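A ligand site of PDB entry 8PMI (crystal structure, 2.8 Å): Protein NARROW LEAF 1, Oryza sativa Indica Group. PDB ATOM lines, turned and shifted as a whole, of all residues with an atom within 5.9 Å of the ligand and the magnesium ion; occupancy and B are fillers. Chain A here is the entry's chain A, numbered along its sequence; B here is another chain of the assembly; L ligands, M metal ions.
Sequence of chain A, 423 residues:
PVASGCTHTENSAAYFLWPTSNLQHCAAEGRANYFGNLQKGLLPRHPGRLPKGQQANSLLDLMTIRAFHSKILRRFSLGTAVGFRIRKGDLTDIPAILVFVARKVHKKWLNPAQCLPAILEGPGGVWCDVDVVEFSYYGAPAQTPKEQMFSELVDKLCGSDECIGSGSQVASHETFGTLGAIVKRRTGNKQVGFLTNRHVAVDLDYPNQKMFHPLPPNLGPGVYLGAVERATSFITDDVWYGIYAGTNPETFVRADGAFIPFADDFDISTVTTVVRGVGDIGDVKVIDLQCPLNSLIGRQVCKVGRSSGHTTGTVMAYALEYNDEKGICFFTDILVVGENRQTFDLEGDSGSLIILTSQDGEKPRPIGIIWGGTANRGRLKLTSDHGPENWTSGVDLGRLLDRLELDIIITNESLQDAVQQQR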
ATOM      1  N   PHE A  76     -21.593   8.509   9.090  1.00  0.00           N
ATOM      2  CA  PHE A  76     -21.884   9.572  10.038  1.00  0.00           C
ATOM      3  C   PHE A  76     -21.697  10.907   9.323  1.00  0.00           C
ATOM      4  O   PHE A  76     -20.609  11.480   9.327  1.00  0.00           O
ATOM      5  CB  PHE A  76     -20.997   9.434  11.266  1.00  0.00           C
ATOM      6  CG  PHE A  76     -20.730   8.007  11.667  1.00  0.00           C
ATOM      7  CD1 PHE A  76     -21.626   7.322  12.477  1.00  0.00           C
ATOM      8  CD2 PHE A  76     -19.598   7.346  11.222  1.00  0.00           C
ATOM      9  CE1 PHE A  76     -21.394   6.005  12.833  1.00  0.00           C
ATOM     10  CE2 PHE A  76     -19.361   6.025  11.587  1.00  0.00           C
ATOM     11  CZ  PHE A  76     -20.254   5.364  12.396  1.00  0.00           C
ATOM     12  N   ARG A  85     -10.926  23.079   1.701  1.00  0.00           N
ATOM     13  CA  ARG A  85     -10.908  22.830   3.133  1.00  0.00           C
ATOM     14  C   ARG A  85     -11.011  24.143   3.897  1.00  0.00           C
ATOM     15  O   ARG A  85     -10.423  25.160   3.505  1.00  0.00           O
ATOM     16  CB  ARG A  85      -9.644  22.078   3.539  1.00  0.00           C
ATOM     17  CG  ARG A  85      -9.386  22.086   5.039  1.00  0.00           C
ATOM     18  CD  ARG A  85      -8.073  21.392   5.395  1.00  0.00           C
ATOM     19  NE  ARG A  85      -8.077  19.992   4.996  1.00  0.00           N
ATOM     20  CZ  ARG A  85      -8.551  19.000   5.745  1.00  0.00           C
ATOM     21  NH1 ARG A  85      -9.063  19.231   6.945  1.00  0.00           N
ATOM     22  NH2 ARG A  85      -8.511  17.754   5.278  1.00  0.00           N
ATOM     23  N   ILE A  86     -11.792  24.136   4.978  1.00  0.00           N
ATOM     24  CA  ILE A  86     -11.890  25.318   5.833  1.00  0.00           C
ATOM     25  C   ILE A  86     -11.236  25.000   7.171  1.00  0.00           C
ATOM     26  O   ILE A  86     -11.871  24.437   8.072  1.00  0.00           O
ATOM     27  CB  ILE A  86     -13.350  25.750   6.030  1.00  0.00           C
ATOM     28  CG1 ILE A  86     -14.054  25.869   4.683  1.00  0.00           C
ATOM     29  CG2 ILE A  86     -13.414  27.071   6.786  1.00  0.00           C
ATOM     30  CD1 ILE A  86     -15.521  26.185   4.801  1.00  0.00           C
ATOM     31  N   ARG A  87      -9.954  25.363   7.295  1.00  0.00           N
ATOM     32  CA  ARG A  87      -9.174  25.164   8.516  1.00  0.00           C
ATOM     33  C   ARG A  87      -9.246  26.413   9.380  1.00  0.00           C
ATOM     34  O   ARG A  87      -8.736  27.476   9.001  1.00  0.00           O
ATOM     35  CB  ARG A  87      -7.730  24.805   8.186  1.00  0.00           C
ATOM     36  CG  ARG A  87      -6.908  24.374   9.399  1.00  0.00           C
ATOM     37  CD  ARG A  87      -5.467  24.056   9.042  1.00  0.00           C
ATOM     38  NE  ARG A  87      -5.320  22.828   8.262  1.00  0.00           N
ATOM     39  CZ  ARG A  87      -4.999  22.776   6.974  1.00  0.00           C
ATOM     40  NH1 ARG A  87      -4.810  23.880   6.265  1.00  0.00           N
ATOM     41  NH2 ARG A  87      -4.866  21.594   6.379  1.00  0.00           N
ATOM     42  N   LYS A  88      -9.884  26.299  10.546  1.00  0.00           N
ATOM     43  CA  LYS A  88      -9.959  27.406  11.500  1.00  0.00           C
ATOM     44  C   LYS A  88     -10.575  28.653  10.868  1.00  0.00           C
ATOM     45  O   LYS A  88      -9.955  29.712  10.763  1.00  0.00           O
ATOM     46  CB  LYS A  88      -8.569  27.707  12.079  1.00  0.00           C
ATOM     47  CG  LYS A  88      -8.114  26.680  13.113  1.00  0.00           C
ATOM     48  CD  LYS A  88      -6.741  27.031  13.667  1.00  0.00           C
ATOM     49  CE  LYS A  88      -6.404  26.186  14.888  1.00  0.00           C
ATOM     50  NZ  LYS A  88      -6.475  24.733  14.582  1.00  0.00           N
ATOM     51  N   GLY A  89     -11.825  28.503  10.437  1.00  0.00           N
ATOM     52  CA  GLY A  89     -12.576  29.615   9.890  1.00  0.00           C
ATOM     53  C   GLY A  89     -12.242  30.028   8.476  1.00  0.00           C
ATOM     54  O   GLY A  89     -13.131  30.053   7.623  1.00  0.00           O
ATOM     55  N   VAL A 101     -21.294  17.559   9.685  1.00  0.00           N
ATOM     56  CA  VAL A 101     -21.701  16.851  10.886  1.00  0.00           C
ATOM     57  C   VAL A 101     -22.580  17.769  11.712  1.00  0.00           C
ATOM     58  O   VAL A 101     -22.581  18.995  11.551  1.00  0.00           O
ATOM     59  CB  VAL A 101     -20.490  16.360  11.713  1.00  0.00           C
ATOM     60  CG1 VAL A 101     -19.619  15.423  10.880  1.00  0.00           C
ATOM     61  CG2 VAL A 101     -19.692  17.548  12.215  1.00  0.00           C
ATOM     62  N   ARG A 103     -22.452  18.165  15.064  1.00  0.00           N
ATOM     63  CA  ARG A 103     -21.681  18.823  16.104  1.00  0.00           C
ATOM     64  C   ARG A 103     -20.250  18.322  16.046  1.00  0.00           C
ATOM     65  O   ARG A 103     -19.996  17.132  16.265  1.00  0.00           O
ATOM     66  CB  ARG A 103     -22.279  18.544  17.491  1.00  0.00           C
ATOM     67  CG  ARG A 103     -21.679  19.377  18.615  1.00  0.00           C
ATOM     68  CD  ARG A 103     -22.537  19.279  19.866  1.00  0.00           C
ATOM     69  NE  ARG A 103     -22.184  20.290  20.859  1.00  0.00           N
ATOM     70  CZ  ARG A 103     -22.915  20.556  21.928  1.00  0.00           C
ATOM     71  NH1 ARG A 103     -24.050  19.919  22.184  1.00  0.00           N
ATOM     72  NH2 ARG A 103     -22.496  21.496  22.779  1.00  0.00           N
ATOM     73  N   LYS A 104     -19.313  19.230  15.761  1.00  0.00           N
ATOM     74  CA  LYS A 104     -17.894  18.916  15.745  1.00  0.00           C
ATOM     75  C   LYS A 104     -17.365  18.878  17.174  1.00  0.00           C
ATOM     76  O   LYS A 104     -17.440  19.886  17.894  1.00  0.00           O
ATOM     77  CB  LYS A 104     -17.113  19.931  14.931  1.00  0.00           C
ATOM     78  CG  LYS A 104     -17.114  19.675  13.433  1.00  0.00           C
ATOM     79  CD  LYS A 104     -15.703  19.735  12.858  1.00  0.00           C
ATOM     80  CE  LYS A 104     -15.005  21.047  13.179  1.00  0.00           C
ATOM     81  NZ  LYS A 104     -13.625  21.099  12.633  1.00  0.00           N
ATOM     82  N   VAL A 105     -16.821  17.742  17.573  1.00  0.00           N
ATOM     83  CA  VAL A 105     -16.165  17.588  18.861  1.00  0.00           C
ATOM     84  C   VAL A 105     -14.689  17.317  18.619  1.00  0.00           C
ATOM     85  O   VAL A 105     -14.247  17.084  17.490  1.00  0.00           O
ATOM     86  CB  VAL A 105     -16.814  16.479  19.720  1.00  0.00           C
ATOM     87  CG1 VAL A 105     -18.291  16.758  19.914  1.00  0.00           C
ATOM     88  CG2 VAL A 105     -16.604  15.127  19.064  1.00  0.00           C
ATOM     89  N   HIS A 106     -13.912  17.342  19.697  1.00  0.00           N
ATOM     90  CA  HIS A 106     -12.488  17.067  19.566  1.00  0.00           C
ATOM     91  C   HIS A 106     -12.280  15.589  19.250  1.00  0.00           C
ATOM     92  O   HIS A 106     -13.113  14.735  19.553  1.00  0.00           O
ATOM     93  CB  HIS A 106     -11.746  17.449  20.845  1.00  0.00           C
ATOM     94  CG  HIS A 106     -10.255  17.388  20.721  1.00  0.00           C
ATOM     95  ND1 HIS A 106      -9.537  16.219  20.893  1.00  0.00           N
ATOM     96  CD2 HIS A 106      -9.343  18.347  20.446  1.00  0.00           C
ATOM     97  CE1 HIS A 106      -8.250  16.462  20.725  1.00  0.00           C
ATOM     98  NE2 HIS A 106      -8.103  17.747  20.450  1.00  0.00           N
ATOM     99  N   LYS A 107     -11.129  15.297  18.643  1.00  0.00           N
ATOM    100  CA  LYS A 107     -10.889  13.932  18.174  1.00  0.00           C
ATOM    101  C   LYS A 107     -10.852  12.928  19.319  1.00  0.00           C
ATOM    102  O   LYS A 107     -11.100  11.744  19.079  1.00  0.00           O
ATOM    103  CB  LYS A 107      -9.581  13.869  17.376  1.00  0.00           C
ATOM    104  CG  LYS A 107      -9.392  12.554  16.623  1.00  0.00           C
ATOM    105  CD  LYS A 107      -8.202  12.634  15.668  1.00  0.00           C
ATOM    106  CE  LYS A 107      -6.896  12.866  16.420  1.00  0.00           C
ATOM    107  NZ  LYS A 107      -5.723  12.936  15.497  1.00  0.00           N
ATOM    108  N   LYS A 108     -10.566  13.367  20.542  1.00  0.00           N
ATOM    109  CA  LYS A 108     -10.496  12.399  21.635  1.00  0.00           C
ATOM    110  C   LYS A 108     -11.871  11.997  22.151  1.00  0.00           C
ATOM    111  O   LYS A 108     -12.043  10.848  22.580  1.00  0.00           O
ATOM    112  CB  LYS A 108      -9.663  12.961  22.791  1.00  0.00           C
ATOM    113  CG  LYS A 108      -8.266  13.401  22.404  1.00  0.00           C
ATOM    114  CD  LYS A 108      -7.482  13.830  23.631  1.00  0.00           C
ATOM    115  CE  LYS A 108      -8.300  14.774  24.514  1.00  0.00           C
ATOM    116  NZ  LYS A 108      -8.862  15.921  23.745  1.00  0.00           N
ATOM    117  N   LEU A 110     -14.212  10.964  20.483  1.00  0.00           N
ATOM    118  CA  LEU A 110     -14.739  10.385  19.251  1.00  0.00           C
ATOM    119  C   LEU A 110     -14.192   8.972  19.103  1.00  0.00           C
ATOM    120  O   LEU A 110     -12.982   8.800  18.960  1.00  0.00           O
ATOM    121  CB  LEU A 110     -14.355  11.235  18.032  1.00  0.00           C
ATOM    122  CG  LEU A 110     -15.513  11.512  17.079  1.00  0.00           C
ATOM    123  CD1 LEU A 110     -15.040  12.298  15.856  1.00  0.00           C
ATOM    124  CD2 LEU A 110     -16.173  10.211  16.672  1.00  0.00           C
ATOM    125  N   GLN A 114     -16.243   6.286  14.181  1.00  0.00           N
ATOM    126  CA  GLN A 114     -16.989   7.405  13.622  1.00  0.00           C
ATOM    127  C   GLN A 114     -16.105   8.546  13.140  1.00  0.00           C
ATOM    128  O   GLN A 114     -16.616   9.484  12.532  1.00  0.00           O
ATOM    129  CB  GLN A 114     -17.993   7.934  14.668  1.00  0.00           C
ATOM    130  CG  GLN A 114     -19.114   6.959  15.003  1.00  0.00           C
ATOM    131  CD  GLN A 114     -20.071   7.527  16.029  1.00  0.00           C
ATOM    132  OE1 GLN A 114     -19.664   8.247  16.942  1.00  0.00           O
ATOM    133  NE2 GLN A 114     -21.353   7.221  15.872  1.00  0.00           N
ATOM    134  N   CYS A 115     -14.803   8.489  13.397  1.00  0.00           N
ATOM    135  CA  CYS A 115     -13.928   9.574  12.980  1.00  0.00           C
ATOM    136  C   CYS A 115     -13.846   9.641  11.452  1.00  0.00           C
ATOM    137  O   CYS A 115     -14.283   8.722  10.732  1.00  0.00           O
ATOM    138  CB  CYS A 115     -12.530   9.410  13.578  1.00  0.00           C
ATOM    139  SG  CYS A 115     -11.375  10.737  13.181  1.00  0.00           S
ATOM    140  N   LEU A 116     -13.305  10.743  10.942  1.00  0.00           N
ATOM    141  CA  LEU A 116     -13.160  10.952   9.512  1.00  0.00           C
ATOM    142  C   LEU A 116     -11.689  11.091   9.135  1.00  0.00           C
ATOM    143  O   LEU A 116     -10.938  11.786   9.822  1.00  0.00           O
ATOM    144  CB  LEU A 116     -13.922  12.194   9.039  1.00  0.00           C
ATOM    145  CG  LEU A 116     -15.378  11.979   8.636  1.00  0.00           C
ATOM    146  CD1 LEU A 116     -16.171  11.340   9.769  1.00  0.00           C
ATOM    147  CD2 LEU A 116     -16.010  13.288   8.200  1.00  0.00           C
ATOM    148  N   VAL A 130     -10.242  15.876   3.165  1.00  0.00           N
ATOM    149  CA  VAL A 130     -11.560  15.702   3.756  1.00  0.00           C
ATOM    150  C   VAL A 130     -11.663  16.668   4.925  1.00  0.00           C
ATOM    151  O   VAL A 130     -10.931  16.536   5.910  1.00  0.00           O
ATOM    152  CB  VAL A 130     -11.811  14.269   4.250  1.00  0.00           C
ATOM    153  CG1 VAL A 130     -13.115  14.186   4.997  1.00  0.00           C
ATOM    154  CG2 VAL A 130     -11.820  13.304   3.088  1.00  0.00           C
ATOM    155  N   ASP A 131     -12.590  17.616   4.835  1.00  0.00           N
ATOM    156  CA  ASP A 131     -12.792  18.629   5.869  1.00  0.00           C
ATOM    157  C   ASP A 131     -14.142  18.415   6.538  1.00  0.00           C
ATOM    158  O   ASP A 131     -15.131  18.073   5.874  1.00  0.00           O
ATOM    159  CB  ASP A 131     -12.706  20.039   5.267  1.00  0.00           C
ATOM    160  CG  ASP A 131     -12.743  21.131   6.322  1.00  0.00           C
ATOM    161  OD1 ASP A 131     -11.770  21.259   7.094  1.00  0.00           O
ATOM    162  OD2 ASP A 131     -13.750  21.877   6.389  1.00  0.00           O
ATOM    163  N   VAL A 132     -14.186  18.624   7.848  1.00  0.00           N
ATOM    164  CA  VAL A 132     -15.389  18.444   8.643  1.00  0.00           C
ATOM    165  C   VAL A 132     -15.885  19.815   9.081  1.00  0.00           C
ATOM    166  O   VAL A 132     -15.091  20.641   9.552  1.00  0.00           O
ATOM    167  CB  VAL A 132     -15.137  17.539   9.857  1.00  0.00           C
ATOM    168  CG1 VAL A 132     -16.438  17.271  10.595  1.00  0.00           C
ATOM    169  CG2 VAL A 132     -14.480  16.236   9.422  1.00  0.00           C
ATOM    170  N   VAL A 133     -17.175  20.052   8.914  1.00  0.00           N
ATOM    171  CA  VAL A 133     -17.800  21.325   9.269  1.00  0.00           C
ATOM    172  C   VAL A 133     -19.110  21.054  10.011  1.00  0.00           C
ATOM    173  O   VAL A 133     -19.882  20.174   9.627  1.00  0.00           O
ATOM    174  CB  VAL A 133     -18.071  22.179   8.023  1.00  0.00           C
ATOM    175  CG1 VAL A 133     -18.721  23.489   8.430  1.00  0.00           C
ATOM    176  CG2 VAL A 133     -16.782  22.415   7.259  1.00  0.00           C
ATOM    177  N   PRO B 221     -22.281  12.887  19.436  1.00  0.00           N
ATOM    178  CA  PRO B 221     -20.998  12.234  19.729  1.00  0.00           C
ATOM    179  C   PRO B 221     -20.399  12.687  21.051  1.00  0.00           C
ATOM    180  O   PRO B 221     -20.591  13.808  21.514  1.00  0.00           O
ATOM    181  CB  PRO B 221     -20.121  12.676  18.556  1.00  0.00           C
ATOM    182  CG  PRO B 221     -20.634  14.035  18.219  1.00  0.00           C
ATOM    183  CD  PRO B 221     -22.122  14.003  18.486  1.00  0.00           C
HETATM  184  P1  LIG L   1     -10.421  22.997  11.558  1.00  0.00           P
HETATM  185  O1  LIG L   1     -10.990  21.890  12.365  1.00  0.00           O
HETATM  186  O2  LIG L   1     -11.451  23.663  10.625  1.00  0.00           O
HETATM  187  O3  LIG L   1      -9.702  24.085  12.372  1.00  0.00           O
HETATM  188  P2  LIG L   1      -8.952  21.109   9.779  1.00  0.00           P
HETATM  189  O4  LIG L   1      -7.539  20.709   9.968  1.00  0.00           O
HETATM  190  O5  LIG L   1      -9.399  21.326   8.339  1.00  0.00           O
HETATM  191  O6  LIG L   1      -9.302  22.439  10.567  1.00  0.00           O
HETATM  192  P3  LIG L   1     -11.215  19.215   9.976  1.00  0.00           P
HETATM  193  O7  LIG L   1     -10.824  18.129   9.055  1.00  0.00           O
HETATM  194  O8  LIG L   1     -12.241  20.212   9.416  1.00  0.00           O
HETATM  195  O9  LIG L   1      -9.953  20.072  10.441  1.00  0.00           O
HETATM  196  O10 LIG L   1     -11.775  18.615  11.328  1.00  0.00           O
HETATM  197  C1  LIG L   1     -11.385  17.310  11.791  1.00  0.00           C
HETATM  198  C2  LIG L   1     -11.843  17.142  13.221  1.00  0.00           C
HETATM  199  O11 LIG L   1     -13.287  17.102  13.266  1.00  0.00           O
HETATM  200  C3  LIG L   1     -11.390  15.880  13.937  1.00  0.00           C
HETATM  201  O12 LIG L   1     -10.108  16.045  14.531  1.00  0.00           O
HETATM  202  C4  LIG L   1     -12.461  15.714  15.017  1.00  0.00           C
HETATM  203  O13 LIG L   1     -12.205  16.529  16.154  1.00  0.00           O
HETATM  204  C5  LIG L   1     -13.719  16.201  14.284  1.00  0.00           C
HETATM  205  N1  LIG L   1     -14.482  15.137  13.648  1.00  0.00           N
HETATM  206  C6  LIG L   1     -14.047  14.263  12.681  1.00  0.00           C
HETATM  207  N2  LIG L   1     -14.946  13.405  12.286  1.00  0.00           N
HETATM  208  C7  LIG L   1     -16.065  13.733  13.043  1.00  0.00           C
HETATM  209  C8  LIG L   1     -17.366  13.202  13.083  1.00  0.00           C
HETATM  210  N3  LIG L   1     -17.778  12.173  12.333  1.00  0.00           N
HETATM  211  N4  LIG L   1     -18.244  13.762  13.945  1.00  0.00           N
HETATM  212  C9  LIG L   1     -17.840  14.779  14.693  1.00  0.00           C
HETATM  213  N5  LIG L   1     -16.636  15.368  14.738  1.00  0.00           N
HETATM  214  C10 LIG L   1     -15.797  14.793  13.879  1.00  0.00           C
HETATM  215 MG    MG M   1     -11.962  22.446   8.778  1.00  0.00          MG
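The backbone NH of Val 132 sits close to an oxygen (O8) of the ligand (3.0 Å).
The guanidinium group (NE) of Arg 87 is in salt-bridge range of an oxygen (O4) of the ligand (3.5 Å).
The side-chain amino group (NZ) of Lys 88 lies within salt-bridge range of an oxygen (O3) of the ligand.
N of Lys 88 is in hydrogen-bond range of O3 of the ligand, 2.9 Å away.
NH1 of Arg 85 lies within salt-bridge range of O5 of the ligand, 2.5 Å away.
O of Val 105 lies within hydrogen-bond range of O13 of the ligand, 2.5 Å away.
O13 of the ligand is in hydrogen-bond range of N of Lys 107 (3.0 Å).
The backbone carbonyl oxygen (O) of Gln 114 sits at hydrogen-bond distance from a nitrogen (N3) of the ligand (2.9 Å).
A nitrogen (N2) of the ligand is in hydrogen-bond range of the backbone NH of Leu 116 (3.4 Å).
The side-chain amino group (NZ) of Lys 104 is in salt-bridge range of an oxygen (O1) of the ligand (2.8 Å).
The backbone NH (N) of Val 101 sits at hydrogen-bond distance from the backbone carbonyl oxygen (O) of Val 133 (3.0 Å).
The side-chain carboxylate (OD1) of Asp 131 lies close to the guanidinium group (NH1) of Arg 85, at 3.4 Å.
The backbone carbonyl oxygen (O) of Val 132 is in hydrogen-bond range of the side-chain amino group (NZ) of Lys 104 (3.4 Å).
A ring nitrogen (ND1) of His 106 is in hydrogen-bond range of the side-chain amino group (NZ) of Lys 108 (2.9 Å).
O of Val 130 sits at hydrogen-bond distance from NH2 of Arg 85, 2.8 Å away.
N of Arg 87 touches the magnesium ion, at 3.8 Å.
Val 132 touches the magnesium ion (O to MG, 3.7 Å).
The magnesium ion is bound by the side-chain carboxylate of Asp 131 (2.1 Å), the backbone carbonyl oxygen of Ile 86 (2.1 Å), an oxygen (O2) of the ligand (2.3 Å) and an oxygen (O8) of the ligand (2.3 Å).
The magnesium ion has four donor atoms within binding distance.
Slightly farther from the magnesium ion lies an oxygen (O5) of the ligand (2.8 Å).
Residues that only touch the ligand: Val 101 (3.7 Å), Arg 103 (3.6 Å), His 106 (3.2 Å), Leu 110 (3.3 Å) and Val 130 (3.5 Å).
Of the 22 residues printed, 16 come within 4 Å of the ligand.
The nearest printed residue that does not touch the ligand is Cys 115 (4.01 Å).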
